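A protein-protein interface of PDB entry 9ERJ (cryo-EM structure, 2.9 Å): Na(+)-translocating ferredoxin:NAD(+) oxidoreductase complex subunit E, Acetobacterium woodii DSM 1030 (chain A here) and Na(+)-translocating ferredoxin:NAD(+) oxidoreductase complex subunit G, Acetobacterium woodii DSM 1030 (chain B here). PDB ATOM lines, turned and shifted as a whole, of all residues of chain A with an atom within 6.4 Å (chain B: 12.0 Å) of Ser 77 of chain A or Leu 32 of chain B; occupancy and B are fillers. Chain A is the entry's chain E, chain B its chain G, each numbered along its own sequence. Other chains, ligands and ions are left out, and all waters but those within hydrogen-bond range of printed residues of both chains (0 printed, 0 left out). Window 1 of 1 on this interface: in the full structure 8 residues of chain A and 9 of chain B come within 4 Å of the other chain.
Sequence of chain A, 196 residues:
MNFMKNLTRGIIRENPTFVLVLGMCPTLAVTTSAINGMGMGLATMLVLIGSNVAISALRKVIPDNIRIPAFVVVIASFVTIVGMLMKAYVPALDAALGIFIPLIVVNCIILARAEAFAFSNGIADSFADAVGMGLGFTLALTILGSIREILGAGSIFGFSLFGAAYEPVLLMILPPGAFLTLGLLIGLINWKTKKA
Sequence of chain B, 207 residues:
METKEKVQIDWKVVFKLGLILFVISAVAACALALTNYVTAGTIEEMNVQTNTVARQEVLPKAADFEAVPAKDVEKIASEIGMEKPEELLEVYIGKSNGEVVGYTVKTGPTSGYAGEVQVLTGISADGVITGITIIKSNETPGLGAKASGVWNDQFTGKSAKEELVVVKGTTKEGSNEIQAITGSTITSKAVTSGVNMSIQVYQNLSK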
ATOM      1  N   VAL A  72      -8.428  19.836  -3.217  1.00  0.00           N
ATOM      2  CA  VAL A  72      -7.081  19.943  -2.664  1.00  0.00           C
ATOM      3  C   VAL A  72      -6.845  18.894  -1.585  1.00  0.00           C
ATOM      4  O   VAL A  72      -5.707  18.467  -1.377  1.00  0.00           O
ATOM      5  CB  VAL A  72      -6.806  21.364  -2.135  1.00  0.00           C
ATOM      6  CG1 VAL A  72      -6.777  22.364  -3.282  1.00  0.00           C
ATOM      7  CG2 VAL A  72      -7.817  21.761  -1.075  1.00  0.00           C
ATOM      8  N   VAL A  73      -7.899  18.450  -0.897  1.00  0.00           N
ATOM      9  CA  VAL A  73      -7.743  17.413   0.122  1.00  0.00           C
ATOM     10  C   VAL A  73      -7.282  16.104  -0.512  1.00  0.00           C
ATOM     11  O   VAL A  73      -6.334  15.463  -0.041  1.00  0.00           O
ATOM     12  CB  VAL A  73      -9.057  17.232   0.907  1.00  0.00           C
ATOM     13  CG1 VAL A  73      -9.044  15.928   1.684  1.00  0.00           C
ATOM     14  CG2 VAL A  73      -9.276  18.405   1.844  1.00  0.00           C
ATOM     15  N   VAL A  74      -7.934  15.704  -1.607  1.00  0.00           N
ATOM     16  CA  VAL A  74      -7.556  14.478  -2.307  1.00  0.00           C
ATOM     17  C   VAL A  74      -6.148  14.597  -2.877  1.00  0.00           C
ATOM     18  O   VAL A  74      -5.326  13.670  -2.757  1.00  0.00           O
ATOM     19  CB  VAL A  74      -8.585  14.159  -3.406  1.00  0.00           C
ATOM     20  CG1 VAL A  74      -8.336  12.779  -3.985  1.00  0.00           C
ATOM     21  CG2 VAL A  74      -9.998  14.266  -2.859  1.00  0.00           C
ATOM     22  N   ILE A  75      -5.844  15.740  -3.503  1.00  0.00           N
ATOM     23  CA  ILE A  75      -4.523  15.919  -4.102  1.00  0.00           C
ATOM     24  C   ILE A  75      -3.435  15.869  -3.034  1.00  0.00           C
ATOM     25  O   ILE A  75      -2.401  15.211  -3.210  1.00  0.00           O
ATOM     26  CB  ILE A  75      -4.470  17.227  -4.912  1.00  0.00           C
ATOM     27  CG1 ILE A  75      -5.500  17.195  -6.042  1.00  0.00           C
ATOM     28  CG2 ILE A  75      -3.086  17.443  -5.492  1.00  0.00           C
ATOM     29  CD1 ILE A  75      -5.701  18.528  -6.721  1.00  0.00           C
ATOM     30  N   ALA A  76      -3.662  16.535  -1.896  1.00  0.00           N
ATOM     31  CA  ALA A  76      -2.680  16.538  -0.819  1.00  0.00           C
ATOM     32  C   ALA A  76      -2.524  15.163  -0.184  1.00  0.00           C
ATOM     33  O   ALA A  76      -1.415  14.801   0.217  1.00  0.00           O
ATOM     34  CB  ALA A  76      -3.067  17.569   0.240  1.00  0.00           C
ATOM     35  N   SER A  77      -3.608  14.390  -0.077  1.00  0.00           N
ATOM     36  CA  SER A  77      -3.496  13.036   0.460  1.00  0.00           C
ATOM     37  C   SER A  77      -2.624  12.161  -0.433  1.00  0.00           C
ATOM     38  O   SER A  77      -1.739  11.439   0.052  1.00  0.00           O
ATOM     39  CB  SER A  77      -4.886  12.421   0.624  1.00  0.00           C
ATOM     40  OG  SER A  77      -5.829  13.394   1.033  1.00  0.00           O
ATOM     41  N   PHE A  78      -2.850  12.225  -1.750  1.00  0.00           N
ATOM     42  CA  PHE A  78      -2.023  11.442  -2.665  1.00  0.00           C
ATOM     43  C   PHE A  78      -0.567  11.898  -2.631  1.00  0.00           C
ATOM     44  O   PHE A  78       0.354  11.066  -2.639  1.00  0.00           O
ATOM     45  CB  PHE A  78      -2.583  11.518  -4.085  1.00  0.00           C
ATOM     46  CG  PHE A  78      -3.694  10.544  -4.347  1.00  0.00           C
ATOM     47  CD1 PHE A  78      -3.421   9.198  -4.526  1.00  0.00           C
ATOM     48  CD2 PHE A  78      -5.009  10.968  -4.405  1.00  0.00           C
ATOM     49  CE1 PHE A  78      -4.439   8.295  -4.762  1.00  0.00           C
ATOM     50  CE2 PHE A  78      -6.031  10.070  -4.641  1.00  0.00           C
ATOM     51  CZ  PHE A  78      -5.746   8.732  -4.820  1.00  0.00           C
ATOM     52  N   VAL A  79      -0.341  13.214  -2.571  1.00  0.00           N
ATOM     53  CA  VAL A  79       1.020  13.743  -2.514  1.00  0.00           C
ATOM     54  C   VAL A  79       1.724  13.280  -1.243  1.00  0.00           C
ATOM     55  O   VAL A  79       2.896  12.887  -1.276  1.00  0.00           O
ATOM     56  CB  VAL A  79       0.999  15.280  -2.630  1.00  0.00           C
ATOM     57  CG1 VAL A  79       2.323  15.878  -2.188  1.00  0.00           C
ATOM     58  CG2 VAL A  79       0.693  15.694  -4.055  1.00  0.00           C
ATOM     59  N   THR A  80       1.020  13.306  -0.108  1.00  0.00           N
ATOM     60  CA  THR A  80       1.617  12.881   1.156  1.00  0.00           C
ATOM     61  C   THR A  80       1.965  11.397   1.143  1.00  0.00           C
ATOM     62  O   THR A  80       3.031  11.004   1.633  1.00  0.00           O
ATOM     63  CB  THR A  80       0.675  13.198   2.315  1.00  0.00           C
ATOM     64  OG1 THR A  80       0.212  14.549   2.200  1.00  0.00           O
ATOM     65  CG2 THR A  80       1.390  13.029   3.644  1.00  0.00           C
ATOM     66  N   ILE A  81       1.082  10.557   0.591  1.00  0.00           N
ATOM     67  CA  ILE A  81       1.377   9.125   0.527  1.00  0.00           C
ATOM     68  C   ILE A  81       2.593   8.862  -0.358  1.00  0.00           C
ATOM     69  O   ILE A  81       3.497   8.090   0.007  1.00  0.00           O
ATOM     70  CB  ILE A  81       0.139   8.345   0.042  1.00  0.00           C
ATOM     71  CG1 ILE A  81      -0.954   8.367   1.111  1.00  0.00           C
ATOM     72  CG2 ILE A  81       0.506   6.912  -0.306  1.00  0.00           C
ATOM     73  CD1 ILE A  81      -2.310   7.939   0.603  1.00  0.00           C
ATOM     74  N   VAL A  82       2.646   9.515  -1.526  1.00  0.00           N
ATOM     75  CA  VAL A  82       3.778   9.334  -2.434  1.00  0.00           C
ATOM     76  C   VAL A  82       5.070   9.812  -1.780  1.00  0.00           C
ATOM     77  O   VAL A  82       6.119   9.164  -1.895  1.00  0.00           O
ATOM     78  CB  VAL A  82       3.505  10.054  -3.769  1.00  0.00           C
ATOM     79  CG1 VAL A  82       4.786  10.237  -4.567  1.00  0.00           C
ATOM     80  CG2 VAL A  82       2.478   9.282  -4.582  1.00  0.00           C
ATOM     81  N   MET A  84       5.755   9.965   1.484  1.00  0.00           N
ATOM     82  CA  MET A  84       6.148   9.011   2.518  1.00  0.00           C
ATOM     83  C   MET A  84       6.834   7.794   1.913  1.00  0.00           C
ATOM     84  O   MET A  84       7.874   7.347   2.415  1.00  0.00           O
ATOM     85  CB  MET A  84       4.932   8.577   3.338  1.00  0.00           C
ATOM     86  CG  MET A  84       4.491   9.570   4.399  1.00  0.00           C
ATOM     87  SD  MET A  84       2.843   9.198   5.029  1.00  0.00           S
ATOM     88  CE  MET A  84       2.660  10.467   6.275  1.00  0.00           C
ATOM     89  N   LEU B  21     -18.083  17.436   3.215  1.00  0.00           N
ATOM     90  CA  LEU B  21     -16.700  17.854   3.423  1.00  0.00           C
ATOM     91  C   LEU B  21     -16.117  17.179   4.652  1.00  0.00           C
ATOM     92  O   LEU B  21     -15.030  16.586   4.582  1.00  0.00           O
ATOM     93  CB  LEU B  21     -16.618  19.375   3.558  1.00  0.00           C
ATOM     94  CG  LEU B  21     -15.329  20.049   3.078  1.00  0.00           C
ATOM     95  CD1 LEU B  21     -14.768  19.366   1.839  1.00  0.00           C
ATOM     96  CD2 LEU B  21     -15.552  21.531   2.823  1.00  0.00           C
ATOM     97  N   PHE B  22     -16.875  17.185   5.756  1.00  0.00           N
ATOM     98  CA  PHE B  22     -16.461  16.490   6.970  1.00  0.00           C
ATOM     99  C   PHE B  22     -16.078  15.055   6.658  1.00  0.00           C
ATOM    100  O   PHE B  22     -14.946  14.632   6.933  1.00  0.00           O
ATOM    101  CB  PHE B  22     -17.595  16.545   7.999  1.00  0.00           C
ATOM    102  CG  PHE B  22     -17.431  15.589   9.150  1.00  0.00           C
ATOM    103  CD1 PHE B  22     -16.592  15.892  10.206  1.00  0.00           C
ATOM    104  CD2 PHE B  22     -18.135  14.395   9.182  1.00  0.00           C
ATOM    105  CE1 PHE B  22     -16.444  15.017  11.267  1.00  0.00           C
ATOM    106  CE2 PHE B  22     -17.992  13.517  10.239  1.00  0.00           C
ATOM    107  CZ  PHE B  22     -17.145  13.829  11.282  1.00  0.00           C
ATOM    108  N   VAL B  23     -16.967  14.337   5.961  1.00  0.00           N
ATOM    109  CA  VAL B  23     -16.712  12.938   5.643  1.00  0.00           C
ATOM    110  C   VAL B  23     -15.421  12.812   4.856  1.00  0.00           C
ATOM    111  O   VAL B  23     -14.528  12.036   5.230  1.00  0.00           O
ATOM    112  CB  VAL B  23     -17.906  12.336   4.880  1.00  0.00           C
ATOM    113  CG1 VAL B  23     -17.511  11.025   4.222  1.00  0.00           C
ATOM    114  CG2 VAL B  23     -19.083  12.134   5.818  1.00  0.00           C
ATOM    115  N   ILE B  24     -15.254  13.661   3.833  1.00  0.00           N
ATOM    116  CA  ILE B  24     -14.063  13.590   2.993  1.00  0.00           C
ATOM    117  C   ILE B  24     -12.821  13.772   3.848  1.00  0.00           C
ATOM    118  O   ILE B  24     -11.892  12.952   3.803  1.00  0.00           O
ATOM    119  CB  ILE B  24     -14.135  14.633   1.865  1.00  0.00           C
ATOM    120  CG1 ILE B  24     -15.238  14.271   0.870  1.00  0.00           C
ATOM    121  CG2 ILE B  24     -12.796  14.745   1.154  1.00  0.00           C
ATOM    122  CD1 ILE B  24     -15.422  15.287  -0.235  1.00  0.00           C
ATOM    123  N   SER B  25     -12.848  14.780   4.730  1.00  0.00           N
ATOM    124  CA  SER B  25     -11.683  15.053   5.560  1.00  0.00           C
ATOM    125  C   SER B  25     -11.351  13.849   6.421  1.00  0.00           C
ATOM    126  O   SER B  25     -10.191  13.411   6.465  1.00  0.00           O
ATOM    127  CB  SER B  25     -11.926  16.291   6.422  1.00  0.00           C
ATOM    128  OG  SER B  25     -12.334  17.390   5.626  1.00  0.00           O
ATOM    129  N   ALA B  26     -12.380  13.232   7.016  1.00  0.00           N
ATOM    130  CA  ALA B  26     -12.145  12.070   7.863  1.00  0.00           C
ATOM    131  C   ALA B  26     -11.466  10.967   7.071  1.00  0.00           C
ATOM    132  O   ALA B  26     -10.447  10.416   7.511  1.00  0.00           O
ATOM    133  CB  ALA B  26     -13.461  11.578   8.462  1.00  0.00           C
ATOM    134  N   VAL B  27     -11.953  10.719   5.850  1.00  0.00           N
ATOM    135  CA  VAL B  27     -11.392   9.651   5.033  1.00  0.00           C
ATOM    136  C   VAL B  27      -9.918   9.913   4.776  1.00  0.00           C
ATOM    137  O   VAL B  27      -9.085   9.004   4.894  1.00  0.00           O
ATOM    138  CB  VAL B  27     -12.188   9.500   3.724  1.00  0.00           C
ATOM    139  CG1 VAL B  27     -11.497   8.522   2.786  1.00  0.00           C
ATOM    140  CG2 VAL B  27     -13.606   9.044   4.022  1.00  0.00           C
ATOM    141  N   ALA B  28      -9.564  11.180   4.516  1.00  0.00           N
ATOM    142  CA  ALA B  28      -8.167  11.517   4.275  1.00  0.00           C
ATOM    143  C   ALA B  28      -7.308  11.130   5.467  1.00  0.00           C
ATOM    144  O   ALA B  28      -6.305  10.420   5.314  1.00  0.00           O
ATOM    145  CB  ALA B  28      -8.028  13.007   3.966  1.00  0.00           C
ATOM    146  N   ALA B  29      -7.747  11.501   6.675  1.00  0.00           N
ATOM    147  CA  ALA B  29      -6.988  11.135   7.863  1.00  0.00           C
ATOM    148  C   ALA B  29      -6.933   9.624   8.011  1.00  0.00           C
ATOM    149  O   ALA B  29      -5.868   9.061   8.299  1.00  0.00           O
ATOM    150  CB  ALA B  29      -7.599  11.785   9.103  1.00  0.00           C
ATOM    151  N   CYS B  30      -8.050   8.948   7.709  1.00  0.00           N
ATOM    152  CA  CYS B  30      -8.116   7.499   7.862  1.00  0.00           C
ATOM    153  C   CYS B  30      -7.106   6.811   6.953  1.00  0.00           C
ATOM    154  O   CYS B  30      -6.692   5.676   7.217  1.00  0.00           O
ATOM    155  CB  CYS B  30      -9.537   7.010   7.576  1.00  0.00           C
ATOM    156  SG  CYS B  30      -9.764   5.214   7.554  1.00  0.00           S
ATOM    157  N   ALA B  31      -6.674   7.492   5.890  1.00  0.00           N
ATOM    158  CA  ALA B  31      -5.566   6.958   5.111  1.00  0.00           C
ATOM    159  C   ALA B  31      -4.231   7.285   5.767  1.00  0.00           C
ATOM    160  O   ALA B  31      -3.461   6.374   6.106  1.00  0.00           O
ATOM    161  CB  ALA B  31      -5.614   7.503   3.685  1.00  0.00           C
ATOM    162  N   LEU B  32      -3.982   8.575   6.023  1.00  0.00           N
ATOM    163  CA  LEU B  32      -2.613   9.053   6.209  1.00  0.00           C
ATOM    164  C   LEU B  32      -1.952   8.414   7.421  1.00  0.00           C
ATOM    165  O   LEU B  32      -0.839   7.880   7.316  1.00  0.00           O
ATOM    166  CB  LEU B  32      -2.602  10.578   6.333  1.00  0.00           C
ATOM    167  CG  LEU B  32      -2.919  11.369   5.063  1.00  0.00           C
ATOM    168  CD1 LEU B  32      -2.585  12.837   5.249  1.00  0.00           C
ATOM    169  CD2 LEU B  32      -2.170  10.799   3.870  1.00  0.00           C
ATOM    170  N   ALA B  33      -2.650   8.411   8.560  1.00  0.00           N
ATOM    171  CA  ALA B  33      -2.108   7.826   9.782  1.00  0.00           C
ATOM    172  C   ALA B  33      -1.689   6.380   9.557  1.00  0.00           C
ATOM    173  O   ALA B  33      -0.598   5.970   9.978  1.00  0.00           O
ATOM    174  CB  ALA B  33      -3.135   7.923  10.909  1.00  0.00           C
ATOM    175  N   LEU B  34      -2.517   5.612   8.835  1.00  0.00           N
ATOM    176  CA  LEU B  34      -2.180   4.218   8.571  1.00  0.00           C
ATOM    177  C   LEU B  34      -0.854   4.108   7.835  1.00  0.00           C
ATOM    178  O   LEU B  34       0.019   3.327   8.234  1.00  0.00           O
ATOM    179  CB  LEU B  34      -3.293   3.541   7.772  1.00  0.00           C
ATOM    180  CG  LEU B  34      -4.650   3.395   8.458  1.00  0.00           C
ATOM    181  CD1 LEU B  34      -5.553   2.478   7.652  1.00  0.00           C
ATOM    182  CD2 LEU B  34      -4.474   2.861   9.868  1.00  0.00           C
ATOM    183  N   THR B  35      -0.658   4.939   6.804  1.00  0.00           N
ATOM    184  CA  THR B  35       0.610   4.923   6.085  1.00  0.00           C
ATOM    185  C   THR B  35       1.758   5.270   7.020  1.00  0.00           C
ATOM    186  O   THR B  35       2.814   4.624   6.986  1.00  0.00           O
ATOM    187  CB  THR B  35       0.565   5.892   4.904  1.00  0.00           C
ATOM    188  OG1 THR B  35      -0.742   5.871   4.318  1.00  0.00           O
ATOM    189  CG2 THR B  35       1.590   5.496   3.854  1.00  0.00           C
ATOM    190  N   ASN B  36       1.536   6.243   7.910  1.00  0.00           N
ATOM    191  CA  ASN B  36       2.555   6.605   8.885  1.00  0.00           C
ATOM    192  C   ASN B  36       2.914   5.410   9.755  1.00  0.00           C
ATOM    193  O   ASN B  36       4.097   5.151  10.013  1.00  0.00           O
ATOM    194  CB  ASN B  36       2.064   7.771   9.740  1.00  0.00           C
ATOM    195  CG  ASN B  36       3.059   8.177  10.802  1.00  0.00           C
ATOM    196  OD1 ASN B  36       4.222   8.439  10.507  1.00  0.00           O
ATOM    197  ND2 ASN B  36       2.606   8.232  12.048  1.00  0.00           N
ATOM    198  N   TYR B  37       1.904   4.627  10.151  1.00  0.00           N
ATOM    199  CA  TYR B  37       2.144   3.483  11.024  1.00  0.00           C
ATOM    200  C   TYR B  37       3.016   2.443  10.332  1.00  0.00           C
ATOM    201  O   TYR B  37       3.712   1.663  10.992  1.00  0.00           O
ATOM    202  CB  TYR B  37       0.805   2.885  11.463  1.00  0.00           C
ATOM    203  CG  TYR B  37       0.877   1.941  12.644  1.00  0.00           C
ATOM    204  CD1 TYR B  37       1.224   0.606  12.481  1.00  0.00           C
ATOM    205  CD2 TYR B  37       0.595   2.391  13.927  1.00  0.00           C
ATOM    206  CE1 TYR B  37       1.288  -0.253  13.562  1.00  0.00           C
ATOM    207  CE2 TYR B  37       0.656   1.540  15.013  1.00  0.00           C
ATOM    208  CZ  TYR B  37       1.004   0.220  14.825  1.00  0.00           C
ATOM    209  OH  TYR B  37       1.066  -0.630  15.905  1.00  0.00           O
ATOM    210  N   VAL B  38       3.014   2.434   8.997  1.00  0.00           N
ATOM    211  CA  VAL B  38       3.831   1.467   8.275  1.00  0.00           C
ATOM    212  C   VAL B  38       5.210   2.050   7.981  1.00  0.00           C
ATOM    213  O   VAL B  38       6.185   1.312   7.793  1.00  0.00           O
ATOM    214  CB  VAL B  38       3.102   1.024   6.992  1.00  0.00           C
ATOM    215  CG1 VAL B  38       3.834  -0.120   6.300  1.00  0.00           C
ATOM    216  CG2 VAL B  38       1.672   0.619   7.313  1.00  0.00           C
ATOM    217  N   THR B  39       5.326   3.378   7.973  1.00  0.00           N
ATOM    218  CA  THR B  39       6.496   3.998   7.361  1.00  0.00           C
ATOM    219  C   THR B  39       7.505   4.551   8.358  1.00  0.00           C
ATOM    220  O   THR B  39       8.687   4.183   8.288  1.00  0.00           O
ATOM    221  CB  THR B  39       6.052   5.122   6.422  1.00  0.00           C
ATOM    222  OG1 THR B  39       4.926   4.685   5.652  1.00  0.00           O
ATOM    223  CG2 THR B  39       7.175   5.504   5.485  1.00  0.00           C
ATOM    224  N   ALA B  40       7.052   5.388   9.302  1.00  0.00           N
ATOM    225  CA  ALA B  40       7.936   6.323  10.000  1.00  0.00           C
ATOM    226  C   ALA B  40       9.113   5.625  10.666  1.00  0.00           C
ATOM    227  O   ALA B  40      10.273   5.989  10.424  1.00  0.00           O
ATOM    228  CB  ALA B  40       7.142   7.118  11.035  1.00  0.00           C
ATOM    229  N   GLY B  41       8.837   4.598  11.474  1.00  0.00           N
ATOM    230  CA  GLY B  41       9.904   3.910  12.184  1.00  0.00           C
ATOM    231  C   GLY B  41      10.964   3.357  11.253  1.00  0.00           C
ATOM    232  O   GLY B  41      12.164   3.497  11.517  1.00  0.00           O
ATOM    233  N   ILE B  43      11.905   4.554   8.398  1.00  0.00           N
ATOM    234  CA  ILE B  43      12.741   5.682   7.996  1.00  0.00           C
ATOM    235  C   ILE B  43      13.801   5.947   9.053  1.00  0.00           C
ATOM    236  O   ILE B  43      14.994   6.074   8.741  1.00  0.00           O
ATOM    237  CB  ILE B  43      11.877   6.930   7.743  1.00  0.00           C
ATOM    238  CG1 ILE B  43      10.858   6.668   6.633  1.00  0.00           C
ATOM    239  CG2 ILE B  43      12.752   8.123   7.393  1.00  0.00           C
ATOM    240  CD1 ILE B  43       9.927   7.834   6.383  1.00  0.00           C
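O of Thr 35 of chain B sits at hydrogen-bond distance from OG1 of Thr 39 of chain B, 2.5 Å away.
Among the printed residues, pairs that only touch across the chains: Met 84 of chain A with Thr 39 of chain B (3.6 Å), Ser 77 of chain A with Ala 28 of chain B (3.7 Å), Val 73 of chain A with Ala 28 of chain B (3.8 Å), Ile 81 of chain A with Leu 32 of chain B (3.9 Å), Ser 77 of chain A with Leu 32 of chain B (3.9 Å) and Val 73 of chain A with Ile 24 of chain B (3.97 Å).
Of chain B, only Ala 28 (3.7 Å) and Leu 32 (3.9 Å) come within 4 Å of Ser 77 of chain A. Leu 32 of chain B touches just these residues of chain A: Ser 77 (3.9 Å) and Ile 81 (3.9 Å). Val 73 of chain A touches two residues of chain B. No residue of chain B comes within 4 Å of Val 74 of chain A. No residue of chain B comes within 4 Å of Val 79 of chain A. No residue of chain B comes within 4 Å of Thr 80 of chain A. Of the printed residues of chain B, Met 84 of chain A touches Thr 39 (3.6 Å). Of the printed residues of chain A, Ala 28 of chain B touches Val 73 (3.8 Å) and Ser 77 (3.7 Å). Printed residues of chain A within 4 Å of Thr 39 of chain B: Met 84 (3.6 Å). Of the printed residues of chain A, Ile 24 of chain B touches Val 73 (3.97 Å). Thr 35 of chain B touches none of the printed residues of chain A. Val 38 of chain B touches none of the printed residues of chain A. The nearest residue of chain A that does not touch Leu 32 of chain B is Thr 80 of chain A (4.03 Å).
Hydrophobic or aromatic side chains of chain B that line the printed part of chain A: Ile 24, Ala 28 and Leu 32. Of the 12 printed residues of chain A, 4 touch a printed residue of chain B. Printed residues of chain A that touch a printed residue of chain B: Val 73, Ser 77, Ile 81 and Met 84. Among the printed residues, 6 pairs touch across the chains. Among the printed residues, no Asp or Glu carboxylate lies within 4 Å of a Lys or Arg side-chain nitrogen of the other chain.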
